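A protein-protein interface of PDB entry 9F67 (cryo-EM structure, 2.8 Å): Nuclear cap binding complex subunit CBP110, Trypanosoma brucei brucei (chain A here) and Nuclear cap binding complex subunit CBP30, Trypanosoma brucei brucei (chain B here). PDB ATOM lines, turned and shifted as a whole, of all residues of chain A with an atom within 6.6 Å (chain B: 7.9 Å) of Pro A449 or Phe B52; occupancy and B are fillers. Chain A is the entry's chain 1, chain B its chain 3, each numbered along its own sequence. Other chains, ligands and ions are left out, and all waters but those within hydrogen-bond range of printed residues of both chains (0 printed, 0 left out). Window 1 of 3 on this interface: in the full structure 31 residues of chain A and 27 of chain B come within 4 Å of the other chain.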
ATOM      1  N   SER A 380      -5.599  10.663 -38.837  1.00  0.00           N
ATOM      2  CA  SER A 380      -6.928  10.553 -38.253  1.00  0.00           C
ATOM      3  C   SER A 380      -7.352   9.099 -38.125  1.00  0.00           C
ATOM      4  O   SER A 380      -7.944   8.710 -37.115  1.00  0.00           O
ATOM      5  CB  SER A 380      -7.934  11.336 -39.092  1.00  0.00           C
ATOM      6  OG  SER A 380      -7.563  12.699 -39.187  1.00  0.00           O
ATOM      7  N   ALA A 383      -5.399   7.487 -35.178  1.00  0.00           N
ATOM      8  CA  ALA A 383      -5.946   7.914 -33.898  1.00  0.00           C
ATOM      9  C   ALA A 383      -7.328   7.322 -33.662  1.00  0.00           C
ATOM     10  O   ALA A 383      -7.678   7.002 -32.521  1.00  0.00           O
ATOM     11  CB  ALA A 383      -5.983   9.437 -33.828  1.00  0.00           C
ATOM     12  N   ASN A 384      -8.115   7.158 -34.726  1.00  0.00           N
ATOM     13  CA  ASN A 384      -9.404   6.491 -34.614  1.00  0.00           C
ATOM     14  C   ASN A 384      -9.235   5.058 -34.142  1.00  0.00           C
ATOM     15  O   ASN A 384      -9.980   4.591 -33.275  1.00  0.00           O
ATOM     16  CB  ASN A 384     -10.113   6.530 -35.965  1.00  0.00           C
ATOM     17  CG  ASN A 384     -11.590   6.271 -35.858  1.00  0.00           C
ATOM     18  OD1 ASN A 384     -12.076   5.773 -34.844  1.00  0.00           O
ATOM     19  ND2 ASN A 384     -12.323   6.614 -36.908  1.00  0.00           N
ATOM     20  N   VAL A 387      -8.130   5.023 -30.426  1.00  0.00           N
ATOM     21  CA  VAL A 387      -9.294   5.285 -29.526  1.00  0.00           C
ATOM     22  C   VAL A 387     -10.196   4.042 -29.501  1.00  0.00           C
ATOM     23  O   VAL A 387     -10.564   3.604 -28.389  1.00  0.00           O
ATOM     24  CB  VAL A 387     -10.077   6.536 -29.969  1.00  0.00           C
ATOM     25  CG1 VAL A 387     -11.401   6.675 -29.226  1.00  0.00           C
ATOM     26  CG2 VAL A 387      -9.245   7.803 -29.828  1.00  0.00           C
ATOM     27  N   GLN A 391     -11.390   2.180 -26.155  1.00  0.00           N
ATOM     28  CA  GLN A 391     -12.799   2.102 -25.792  1.00  0.00           C
ATOM     29  C   GLN A 391     -13.278   0.663 -25.705  1.00  0.00           C
ATOM     30  O   GLN A 391     -14.128   0.342 -24.870  1.00  0.00           O
ATOM     31  CB  GLN A 391     -13.646   2.879 -26.795  1.00  0.00           C
ATOM     32  CG  GLN A 391     -13.467   4.377 -26.744  1.00  0.00           C
ATOM     33  CD  GLN A 391     -14.099   4.989 -25.518  1.00  0.00           C
ATOM     34  OE1 GLN A 391     -15.265   5.374 -25.537  1.00  0.00           O
ATOM     35  NE2 GLN A 391     -13.330   5.089 -24.442  1.00  0.00           N
ATOM     36  N   LEU A 441      -4.423  10.592 -22.451  1.00  0.00           N
ATOM     37  CA  LEU A 441      -5.310  11.745 -22.377  1.00  0.00           C
ATOM     38  C   LEU A 441      -4.534  13.026 -22.120  1.00  0.00           C
ATOM     39  O   LEU A 441      -4.853  14.075 -22.691  1.00  0.00           O
ATOM     40  CB  LEU A 441      -6.360  11.529 -21.294  1.00  0.00           C
ATOM     41  CG  LEU A 441      -7.570  10.699 -21.704  1.00  0.00           C
ATOM     42  CD1 LEU A 441      -8.344  10.264 -20.481  1.00  0.00           C
ATOM     43  CD2 LEU A 441      -8.452  11.489 -22.638  1.00  0.00           C
ATOM     44  N   VAL A 444      -3.365  14.141 -25.246  1.00  0.00           N
ATOM     45  CA  VAL A 444      -4.483  14.586 -26.134  1.00  0.00           C
ATOM     46  C   VAL A 444      -5.253  15.713 -25.430  1.00  0.00           C
ATOM     47  O   VAL A 444      -6.346  16.070 -25.911  1.00  0.00           O
ATOM     48  CB  VAL A 444      -5.409  13.438 -26.588  1.00  0.00           C
ATOM     49  CG1 VAL A 444      -4.635  12.363 -27.333  1.00  0.00           C
ATOM     50  CG2 VAL A 444      -6.199  12.826 -25.446  1.00  0.00           C
ATOM     51  N   GLU A 447      -8.883  15.432 -23.572  1.00  0.00           N
ATOM     52  CA  GLU A 447     -10.106  15.439 -24.397  1.00  0.00           C
ATOM     53  C   GLU A 447     -10.458  13.994 -24.781  1.00  0.00           C
ATOM     54  O   GLU A 447      -9.533  13.213 -24.803  1.00  0.00           O
ATOM     55  CB  GLU A 447      -9.827  16.410 -25.529  1.00  0.00           C
ATOM     56  CG  GLU A 447      -9.654  17.852 -25.079  1.00  0.00           C
ATOM     57  CD  GLU A 447      -9.675  18.770 -26.273  1.00  0.00           C
ATOM     58  OE1 GLU A 447      -9.890  18.263 -27.385  1.00  0.00           O
ATOM     59  OE2 GLU A 447      -9.462  19.980 -26.088  1.00  0.00           O
ATOM     60  N   TRP A 448     -11.674  13.662 -25.189  1.00  0.00           N
ATOM     61  CA  TRP A 448     -12.147  12.300 -25.373  1.00  0.00           C
ATOM     62  C   TRP A 448     -13.638  12.339 -25.673  1.00  0.00           C
ATOM     63  O   TRP A 448     -14.305  13.328 -25.346  1.00  0.00           O
ATOM     64  CB  TRP A 448     -11.864  11.481 -24.113  1.00  0.00           C
ATOM     65  CG  TRP A 448     -11.746  10.012 -24.312  1.00  0.00           C
ATOM     66  CD1 TRP A 448     -12.619   9.061 -23.889  1.00  0.00           C
ATOM     67  CD2 TRP A 448     -10.681   9.317 -24.963  1.00  0.00           C
ATOM     68  NE1 TRP A 448     -12.172   7.817 -24.241  1.00  0.00           N
ATOM     69  CE2 TRP A 448     -10.981   7.948 -24.903  1.00  0.00           C
ATOM     70  CE3 TRP A 448      -9.503   9.721 -25.593  1.00  0.00           C
ATOM     71  CZ2 TRP A 448     -10.151   6.981 -25.449  1.00  0.00           C
ATOM     72  CZ3 TRP A 448      -8.682   8.761 -26.135  1.00  0.00           C
ATOM     73  CH2 TRP A 448      -9.008   7.409 -26.060  1.00  0.00           C
ATOM     74  N   PRO A 449     -14.201  11.307 -26.290  1.00  0.00           N
ATOM     75  CA  PRO A 449     -15.661  11.213 -26.364  1.00  0.00           C
ATOM     76  C   PRO A 449     -16.257  10.899 -25.002  1.00  0.00           C
ATOM     77  O   PRO A 449     -16.740   9.786 -24.777  1.00  0.00           O
ATOM     78  CB  PRO A 449     -15.893  10.067 -27.355  1.00  0.00           C
ATOM     79  CG  PRO A 449     -14.608   9.912 -28.080  1.00  0.00           C
ATOM     80  CD  PRO A 449     -13.545  10.282 -27.114  1.00  0.00           C
ATOM     81  N   TRP A 450     -16.221  11.870 -24.086  1.00  0.00           N
ATOM     82  CA  TRP A 450     -16.599  11.601 -22.703  1.00  0.00           C
ATOM     83  C   TRP A 450     -18.074  11.243 -22.586  1.00  0.00           C
ATOM     84  O   TRP A 450     -18.431  10.238 -21.957  1.00  0.00           O
ATOM     85  CB  TRP A 450     -16.273  12.806 -21.826  1.00  0.00           C
ATOM     86  CG  TRP A 450     -14.824  12.954 -21.505  1.00  0.00           C
ATOM     87  CD1 TRP A 450     -14.017  13.989 -21.850  1.00  0.00           C
ATOM     88  CD2 TRP A 450     -14.010  12.039 -20.769  1.00  0.00           C
ATOM     89  NE1 TRP A 450     -12.750  13.777 -21.379  1.00  0.00           N
ATOM     90  CE2 TRP A 450     -12.720  12.583 -20.710  1.00  0.00           C
ATOM     91  CE3 TRP A 450     -14.248  10.807 -20.158  1.00  0.00           C
ATOM     92  CZ2 TRP A 450     -11.672  11.945 -20.067  1.00  0.00           C
ATOM     93  CZ3 TRP A 450     -13.207  10.176 -19.521  1.00  0.00           C
ATOM     94  CH2 TRP A 450     -11.936  10.743 -19.480  1.00  0.00           C
ATOM     95  N   SER A 451     -18.947  12.053 -23.185  1.00  0.00           N
ATOM     96  CA  SER A 451     -20.380  11.830 -23.042  1.00  0.00           C
ATOM     97  C   SER A 451     -20.796  10.509 -23.669  1.00  0.00           C
ATOM     98  O   SER A 451     -21.555   9.737 -23.072  1.00  0.00           O
ATOM     99  CB  SER A 451     -21.152  12.990 -23.666  1.00  0.00           C
ATOM    100  OG  SER A 451     -20.533  13.418 -24.867  1.00  0.00           O
ATOM    101  N   GLU A 452     -20.303  10.230 -24.876  1.00  0.00           N
ATOM    102  CA  GLU A 452     -20.666   8.993 -25.558  1.00  0.00           C
ATOM    103  C   GLU A 452     -20.161   7.775 -24.798  1.00  0.00           C
ATOM    104  O   GLU A 452     -20.894   6.791 -24.622  1.00  0.00           O
ATOM    105  CB  GLU A 452     -20.116   9.008 -26.981  1.00  0.00           C
ATOM    106  CG  GLU A 452     -20.516  10.231 -27.787  1.00  0.00           C
ATOM    107  CD  GLU A 452     -19.557  11.389 -27.622  1.00  0.00           C
ATOM    108  OE1 GLU A 452     -18.962  11.521 -26.533  1.00  0.00           O
ATOM    109  OE2 GLU A 452     -19.402  12.175 -28.578  1.00  0.00           O
ATOM    110  N   SER A 453     -18.915   7.830 -24.326  1.00  0.00           N
ATOM    111  CA  SER A 453     -18.361   6.713 -23.574  1.00  0.00           C
ATOM    112  C   SER A 453     -19.145   6.470 -22.295  1.00  0.00           C
ATOM    113  O   SER A 453     -19.460   5.322 -21.965  1.00  0.00           O
ATOM    114  CB  SER A 453     -16.890   6.968 -23.263  1.00  0.00           C
ATOM    115  OG  SER A 453     -16.681   8.308 -22.858  1.00  0.00           O
ATOM    116  N   LEU A 454     -19.476   7.535 -21.564  1.00  0.00           N
ATOM    117  CA  LEU A 454     -20.223   7.358 -20.325  1.00  0.00           C
ATOM    118  C   LEU A 454     -21.618   6.815 -20.590  1.00  0.00           C
ATOM    119  O   LEU A 454     -22.096   5.937 -19.863  1.00  0.00           O
ATOM    120  CB  LEU A 454     -20.303   8.674 -19.559  1.00  0.00           C
ATOM    121  CG  LEU A 454     -20.872   8.533 -18.150  1.00  0.00           C
ATOM    122  CD1 LEU A 454     -20.032   7.564 -17.349  1.00  0.00           C
ATOM    123  CD2 LEU A 454     -20.939   9.878 -17.463  1.00  0.00           C
ATOM    124  N   PHE A 482     -15.011   5.231 -14.397  1.00  0.00           N
ATOM    125  CA  PHE A 482     -14.732   6.615 -14.752  1.00  0.00           C
ATOM    126  C   PHE A 482     -14.222   7.409 -13.561  1.00  0.00           C
ATOM    127  O   PHE A 482     -13.414   8.326 -13.736  1.00  0.00           O
ATOM    128  CB  PHE A 482     -15.970   7.257 -15.367  1.00  0.00           C
ATOM    129  CG  PHE A 482     -16.128   6.953 -16.822  1.00  0.00           C
ATOM    130  CD1 PHE A 482     -16.734   5.785 -17.236  1.00  0.00           C
ATOM    131  CD2 PHE A 482     -15.635   7.817 -17.779  1.00  0.00           C
ATOM    132  CE1 PHE A 482     -16.863   5.496 -18.570  1.00  0.00           C
ATOM    133  CE2 PHE A 482     -15.760   7.530 -19.113  1.00  0.00           C
ATOM    134  CZ  PHE A 482     -16.375   6.368 -19.509  1.00  0.00           C
ATOM    135  N   PHE A 506     -21.155  14.468 -16.242  1.00  0.00           N
ATOM    136  CA  PHE A 506     -20.129  14.023 -15.315  1.00  0.00           C
ATOM    137  C   PHE A 506     -20.165  14.783 -14.000  1.00  0.00           C
ATOM    138  O   PHE A 506     -19.229  14.667 -13.203  1.00  0.00           O
ATOM    139  CB  PHE A 506     -18.748  14.167 -15.952  1.00  0.00           C
ATOM    140  CG  PHE A 506     -18.360  13.019 -16.826  1.00  0.00           C
ATOM    141  CD1 PHE A 506     -18.789  12.955 -18.133  1.00  0.00           C
ATOM    142  CD2 PHE A 506     -17.553  12.013 -16.346  1.00  0.00           C
ATOM    143  CE1 PHE A 506     -18.428  11.904 -18.937  1.00  0.00           C
ATOM    144  CE2 PHE A 506     -17.194  10.962 -17.148  1.00  0.00           C
ATOM    145  CZ  PHE A 506     -17.630  10.908 -18.443  1.00  0.00           C
ATOM    146  N   MET B  45      -3.797  18.615 -32.427  1.00  0.00           N
ATOM    147  CA  MET B  45      -5.111  18.394 -31.846  1.00  0.00           C
ATOM    148  C   MET B  45      -6.213  18.365 -32.890  1.00  0.00           C
ATOM    149  O   MET B  45      -7.291  17.828 -32.617  1.00  0.00           O
ATOM    150  CB  MET B  45      -5.407  19.461 -30.799  1.00  0.00           C
ATOM    151  CG  MET B  45      -4.835  19.155 -29.427  1.00  0.00           C
ATOM    152  SD  MET B  45      -5.734  17.886 -28.514  1.00  0.00           S
ATOM    153  CE  MET B  45      -4.950  16.392 -29.106  1.00  0.00           C
ATOM    154  N   THR B  46      -5.976  18.932 -34.072  1.00  0.00           N
ATOM    155  CA  THR B  46      -6.954  18.814 -35.143  1.00  0.00           C
ATOM    156  C   THR B  46      -7.095  17.368 -35.590  1.00  0.00           C
ATOM    157  O   THR B  46      -8.187  16.932 -35.973  1.00  0.00           O
ATOM    158  CB  THR B  46      -6.561  19.708 -36.317  1.00  0.00           C
ATOM    159  OG1 THR B  46      -5.387  19.182 -36.946  1.00  0.00           O
ATOM    160  CG2 THR B  46      -6.282  21.115 -35.837  1.00  0.00           C
ATOM    161  N   VAL B  47      -6.000  16.611 -35.554  1.00  0.00           N
ATOM    162  CA  VAL B  47      -6.059  15.198 -35.903  1.00  0.00           C
ATOM    163  C   VAL B  47      -6.872  14.428 -34.873  1.00  0.00           C
ATOM    164  O   VAL B  47      -7.730  13.610 -35.225  1.00  0.00           O
ATOM    165  CB  VAL B  47      -4.639  14.628 -36.042  1.00  0.00           C
ATOM    166  CG1 VAL B  47      -4.680  13.114 -36.084  1.00  0.00           C
ATOM    167  CG2 VAL B  47      -3.971  15.185 -37.281  1.00  0.00           C
ATOM    168  N   TRP B  48      -6.630  14.683 -33.589  1.00  0.00           N
ATOM    169  CA  TRP B  48      -7.266  13.882 -32.551  1.00  0.00           C
ATOM    170  C   TRP B  48      -8.733  14.246 -32.385  1.00  0.00           C
ATOM    171  O   TRP B  48      -9.563  13.377 -32.100  1.00  0.00           O
ATOM    172  CB  TRP B  48      -6.516  14.042 -31.237  1.00  0.00           C
ATOM    173  CG  TRP B  48      -5.275  13.231 -31.177  1.00  0.00           C
ATOM    174  CD1 TRP B  48      -4.016  13.646 -31.465  1.00  0.00           C
ATOM    175  CD2 TRP B  48      -5.171  11.855 -30.812  1.00  0.00           C
ATOM    176  NE1 TRP B  48      -3.130  12.615 -31.302  1.00  0.00           N
ATOM    177  CE2 TRP B  48      -3.818  11.503 -30.898  1.00  0.00           C
ATOM    178  CE3 TRP B  48      -6.094  10.886 -30.417  1.00  0.00           C
ATOM    179  CZ2 TRP B  48      -3.363  10.228 -30.605  1.00  0.00           C
ATOM    180  CZ3 TRP B  48      -5.641   9.626 -30.126  1.00  0.00           C
ATOM    181  CH2 TRP B  48      -4.290   9.304 -30.222  1.00  0.00           C
ATOM    182  N   ARG B  49      -9.078  15.523 -32.548  1.00  0.00           N
ATOM    183  CA  ARG B  49     -10.483  15.904 -32.485  1.00  0.00           C
ATOM    184  C   ARG B  49     -11.257  15.337 -33.666  1.00  0.00           C
ATOM    185  O   ARG B  49     -12.394  14.874 -33.509  1.00  0.00           O
ATOM    186  CB  ARG B  49     -10.613  17.421 -32.421  1.00  0.00           C
ATOM    187  CG  ARG B  49     -10.296  17.971 -31.053  1.00  0.00           C
ATOM    188  CD  ARG B  49     -10.537  19.451 -30.974  1.00  0.00           C
ATOM    189  NE  ARG B  49      -9.938  20.010 -29.771  1.00  0.00           N
ATOM    190  CZ  ARG B  49      -9.736  21.301 -29.567  1.00  0.00           C
ATOM    191  NH1 ARG B  49     -10.083  22.203 -30.469  1.00  0.00           N
ATOM    192  NH2 ARG B  49      -9.169  21.697 -28.433  1.00  0.00           N
ATOM    193  N   SER B  50     -10.648  15.342 -34.851  1.00  0.00           N
ATOM    194  CA  SER B  50     -11.257  14.677 -35.994  1.00  0.00           C
ATOM    195  C   SER B  50     -11.405  13.184 -35.743  1.00  0.00           C
ATOM    196  O   SER B  50     -12.393  12.572 -36.161  1.00  0.00           O
ATOM    197  CB  SER B  50     -10.430  14.933 -37.251  1.00  0.00           C
ATOM    198  OG  SER B  50     -10.348  16.318 -37.528  1.00  0.00           O
ATOM    199  N   ALA B  51     -10.437  12.577 -35.055  1.00  0.00           N
ATOM    200  CA  ALA B  51     -10.528  11.156 -34.741  1.00  0.00           C
ATOM    201  C   ALA B  51     -11.665  10.866 -33.771  1.00  0.00           C
ATOM    202  O   ALA B  51     -12.389   9.879 -33.933  1.00  0.00           O
ATOM    203  CB  ALA B  51      -9.208  10.664 -34.165  1.00  0.00           C
ATOM    204  N   PHE B  52     -11.822  11.703 -32.747  1.00  0.00           N
ATOM    205  CA  PHE B  52     -12.941  11.541 -31.827  1.00  0.00           C
ATOM    206  C   PHE B  52     -14.267  11.698 -32.556  1.00  0.00           C
ATOM    207  O   PHE B  52     -15.202  10.918 -32.337  1.00  0.00           O
ATOM    208  CB  PHE B  52     -12.845  12.554 -30.689  1.00  0.00           C
ATOM    209  CG  PHE B  52     -11.582  12.460 -29.890  1.00  0.00           C
ATOM    210  CD1 PHE B  52     -10.975  11.242 -29.667  1.00  0.00           C
ATOM    211  CD2 PHE B  52     -11.007  13.592 -29.355  1.00  0.00           C
ATOM    212  CE1 PHE B  52      -9.816  11.161 -28.934  1.00  0.00           C
ATOM    213  CE2 PHE B  52      -9.852  13.515 -28.619  1.00  0.00           C
ATOM    214  CZ  PHE B  52      -9.256  12.297 -28.408  1.00  0.00           C
ATOM    215  N   SER B  53     -14.362  12.696 -33.436  1.00  0.00           N
ATOM    216  CA  SER B  53     -15.587  12.898 -34.200  1.00  0.00           C
ATOM    217  C   SER B  53     -15.874  11.712 -35.107  1.00  0.00           C
ATOM    218  O   SER B  53     -17.032  11.317 -35.272  1.00  0.00           O
ATOM    219  CB  SER B  53     -15.493  14.185 -35.016  1.00  0.00           C
ATOM    220  OG  SER B  53     -15.159  15.287 -34.192  1.00  0.00           O
ATOM    221  N   GLN B  54     -14.838  11.137 -35.714  1.00  0.00           N
ATOM    222  CA  GLN B  54     -15.038   9.986 -36.587  1.00  0.00           C
ATOM    223  C   GLN B  54     -15.461   8.756 -35.799  1.00  0.00           C
ATOM    224  O   GLN B  54     -16.348   8.014 -36.232  1.00  0.00           O
ATOM    225  CB  GLN B  54     -13.765   9.702 -37.379  1.00  0.00           C
ATOM    226  CG  GLN B  54     -13.611  10.551 -38.623  1.00  0.00           C
ATOM    227  CD  GLN B  54     -12.209  10.495 -39.188  1.00  0.00           C
ATOM    228  OE1 GLN B  54     -11.576   9.442 -39.202  1.00  0.00           O
ATOM    229  NE2 GLN B  54     -11.716  11.632 -39.658  1.00  0.00           N
ATOM    230  N   TYR B  55     -14.842   8.521 -34.642  1.00  0.00           N
ATOM    231  CA  TYR B  55     -15.219   7.375 -33.822  1.00  0.00           C
ATOM    232  C   TYR B  55     -16.622   7.524 -33.255  1.00  0.00           C
ATOM    233  O   TYR B  55     -17.297   6.522 -33.014  1.00  0.00           O
ATOM    234  CB  TYR B  55     -14.217   7.179 -32.684  1.00  0.00           C
ATOM    235  CG  TYR B  55     -14.648   6.138 -31.681  1.00  0.00           C
ATOM    236  CD1 TYR B  55     -14.473   4.792 -31.935  1.00  0.00           C
ATOM    237  CD2 TYR B  55     -15.237   6.501 -30.485  1.00  0.00           C
ATOM    238  CE1 TYR B  55     -14.871   3.838 -31.032  1.00  0.00           C
ATOM    239  CE2 TYR B  55     -15.640   5.554 -29.578  1.00  0.00           C
ATOM    240  CZ  TYR B  55     -15.453   4.225 -29.857  1.00  0.00           C
ATOM    241  OH  TYR B  55     -15.851   3.274 -28.953  1.00  0.00           O
ATOM    242  N   THR B  56     -17.058   8.754 -32.988  1.00  0.00           N
ATOM    243  CA  THR B  56     -18.417   8.961 -32.502  1.00  0.00           C
ATOM    244  C   THR B  56     -19.438   8.859 -33.628  1.00  0.00           C
ATOM    245  O   THR B  56     -20.508   8.268 -33.446  1.00  0.00           O
ATOM    246  CB  THR B  56     -18.514  10.318 -31.808  1.00  0.00           C
ATOM    247  OG1 THR B  56     -17.701  10.309 -30.630  1.00  0.00           O
ATOM    248  CG2 THR B  56     -19.951  10.628 -31.423  1.00  0.00           C
ATOM    249  N   LYS B  57     -19.121   9.414 -34.799  1.00  0.00           N
ATOM    250  CA  LYS B  57     -20.071   9.434 -35.907  1.00  0.00           C
ATOM    251  C   LYS B  57     -20.338   8.028 -36.418  1.00  0.00           C
ATOM    252  O   LYS B  57     -21.468   7.532 -36.345  1.00  0.00           O
ATOM    253  CB  LYS B  57     -19.537  10.327 -37.028  1.00  0.00           C
ATOM    254  CG  LYS B  57     -20.516  10.568 -38.157  1.00  0.00           C
ATOM    255  CD  LYS B  57     -20.019  11.667 -39.078  1.00  0.00           C
ATOM    256  CE  LYS B  57     -19.878  12.984 -38.336  1.00  0.00           C
ATOM    257  NZ  LYS B  57     -21.196  13.535 -37.915  1.00  0.00           N
ATOM    258  N   MET B  58     -19.312   7.368 -36.936  1.00  0.00           N
ATOM    259  CA  MET B  58     -19.423   5.942 -37.169  1.00  0.00           C
ATOM    260  C   MET B  58     -19.319   5.211 -35.838  1.00  0.00           C
ATOM    261  O   MET B  58     -19.002   5.802 -34.805  1.00  0.00           O
ATOM    262  CB  MET B  58     -18.371   5.485 -38.177  1.00  0.00           C
ATOM    263  CG  MET B  58     -16.977   5.246 -37.643  1.00  0.00           C
ATOM    264  SD  MET B  58     -16.041   4.250 -38.818  1.00  0.00           S
ATOM    265  CE  MET B  58     -14.380   4.388 -38.180  1.00  0.00           C
ATOM    266  N   LEU B  61     -22.285   6.128 -31.877  1.00  0.00           N
ATOM    267  CA  LEU B  61     -22.261   6.622 -30.508  1.00  0.00           C
ATOM    268  C   LEU B  61     -22.912   7.995 -30.455  1.00  0.00           C
ATOM    269  O   LEU B  61     -22.614   8.860 -31.285  1.00  0.00           O
ATOM    270  CB  LEU B  61     -20.832   6.690 -29.974  1.00  0.00           C
ATOM    271  CG  LEU B  61     -20.136   5.351 -29.728  1.00  0.00           C
ATOM    272  CD1 LEU B  61     -19.147   5.063 -30.837  1.00  0.00           C
ATOM    273  CD2 LEU B  61     -19.447   5.343 -28.380  1.00  0.00           C
ATOM    274  N   THR B  62     -23.803   8.191 -29.487  1.00  0.00           N
ATOM    275  CA  THR B  62     -24.526   9.443 -29.324  1.00  0.00           C
ATOM    276  C   THR B  62     -24.332   9.967 -27.911  1.00  0.00           C
ATOM    277  O   THR B  62     -24.211   9.195 -26.956  1.00  0.00           O
ATOM    278  CB  THR B  62     -26.022   9.270 -29.606  1.00  0.00           C
ATOM    279  OG1 THR B  62     -26.560   8.271 -28.732  1.00  0.00           O
ATOM    280  CG2 THR B  62     -26.249   8.846 -31.045  1.00  0.00           C
ATOM    281  N   LYS B  63     -24.305  11.289 -27.784  1.00  0.00           N
ATOM    282  CA  LYS B  63     -24.120  11.920 -26.490  1.00  0.00           C
ATOM    283  C   LYS B  63     -25.387  11.798 -25.649  1.00  0.00           C
ATOM    284  O   LYS B  63     -26.443  11.368 -26.118  1.00  0.00           O
ATOM    285  CB  LYS B  63     -23.725  13.385 -26.657  1.00  0.00           C
ATOM    286  CG  LYS B  63     -22.496  13.593 -27.512  1.00  0.00           C
ATOM    287  CD  LYS B  63     -22.468  14.973 -28.130  1.00  0.00           C
ATOM    288  CE  LYS B  63     -22.070  16.021 -27.114  1.00  0.00           C
ATOM    289  NZ  LYS B  63     -20.595  16.189 -27.052  1.00  0.00           N
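OE2 of Glu A447 lies within salt-bridge range of NH2 of Arg B49, 2.9 Å away.
The side-chain sulfur of Met B45 lies close to the backbone carbonyl oxygen of Val A444 (3.2 Å).
The side-chain hydroxyl (OG1) of Thr B56 is in hydrogen-bond range of the side-chain carboxylate (OE2) of Glu A452, at 3.3 Å.
The backbone carbonyl oxygen (O) of Thr B56 sits at hydrogen-bond distance from the backbone NH (N) of Leu B61, at 3.2 Å.
NE1 of Trp A448 sits close to NE2 of Gln A391, 3.0 Å away.
The backbone carbonyl oxygen of Pro A449 sits at hydrogen-bond distance from the side-chain hydroxyl of Ser A453, 2.4 Å away.
The side-chain hydroxyl of Ser A451 sits at hydrogen-bond distance from the side-chain carboxylate of Glu A452, 3.0 Å away.
O of Phe B52 is in hydrogen-bond range of OG1 of Thr B56.
The side-chain hydroxyl (OG) of Ser B53 lies within hydrogen-bond range of the backbone carbonyl oxygen (O) of Arg B49, 2.9 Å away.
Among the printed residues, merely in contact across the chains: Ser A380 with Val B47, Ser A380 with Ala B51, Ser A380 with Gln B54, Ala A383 with Trp B48, Ala A383 with Ala B51, Asn A384 with Ala B51, Asn A384 with Gln B54, Asn A384 with Tyr B55, Asn A384 with Met B58, Val A387 with Phe B52, Gln A391 with Tyr B55, Val A444 with Trp B48, Glu A447 with Phe B52, Trp A448 with Phe B52, Pro A449 with Phe B52, Pro A449 with Thr B56, Ser A451 with Lys B63, Glu A452 with Leu B61, Glu A452 with Thr B62 and Glu A452 with Lys B63.
Of the printed residues of chain B, Asn A384 touches Ala B51, Gln B54, Tyr B55 and Met B58.
Pro A449 touches just these residues of chain B: Phe B52 (3.7 Å) and Thr B56 (3.7 Å).
Of the printed residues of chain A, Ala B51 touches Ser A380 (3.8 Å), Ala A383 (3.5 Å) and Asn A384 (3.7 Å).
Phe B52 touches just these residues of chain A: Val A387 (3.5 Å), Glu A447 (3.7 Å), Trp A448 (3.7 Å) and Pro A449 (3.7 Å).
Of the printed residues of chain A, Thr B56 touches Pro A449 (3.7 Å) and Glu A452 (3.3 Å).
Printed residues of chain A within 4 Å of Met B58: Asn A384.
The nearest residue of chain B that does not touch Pro A449 is Tyr B55 (4.2 Å).
The nearest printed residue of chain A that does not touch Trp B48 is Val A387 (4.05 Å).
Of the 17 printed residues of chain A, 11 touch a printed residue of chain B.
Hydrophobic or aromatic side chains of chain A that line the printed part of chain B: Ala A383, Val A387, Val A444, Trp A448 and Pro A449.
Printed residues of chain B that touch a printed residue of chain A: Met B45, Val B47, Trp B48, Arg B49, Ala B51, Phe B52, Gln B54, Tyr B55, Thr B56, Met B58, Leu B61, Thr B62 and Lys B63.
Hydrophobic or aromatic side chains of chain B within 4 Å of the printed part of chain A: Met B45, Val B47, Trp B48, Ala B51, Phe B52, Tyr B55, Met B58 and Leu B61.
Along chain B the printed residues that touch a printed residue of chain A span positions 45 to 63.
Among the printed residues, Asp or Glu carboxylates within 4 Å of a Lys or Arg side-chain nitrogen of the other chain: Glu A447 with Arg B49.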
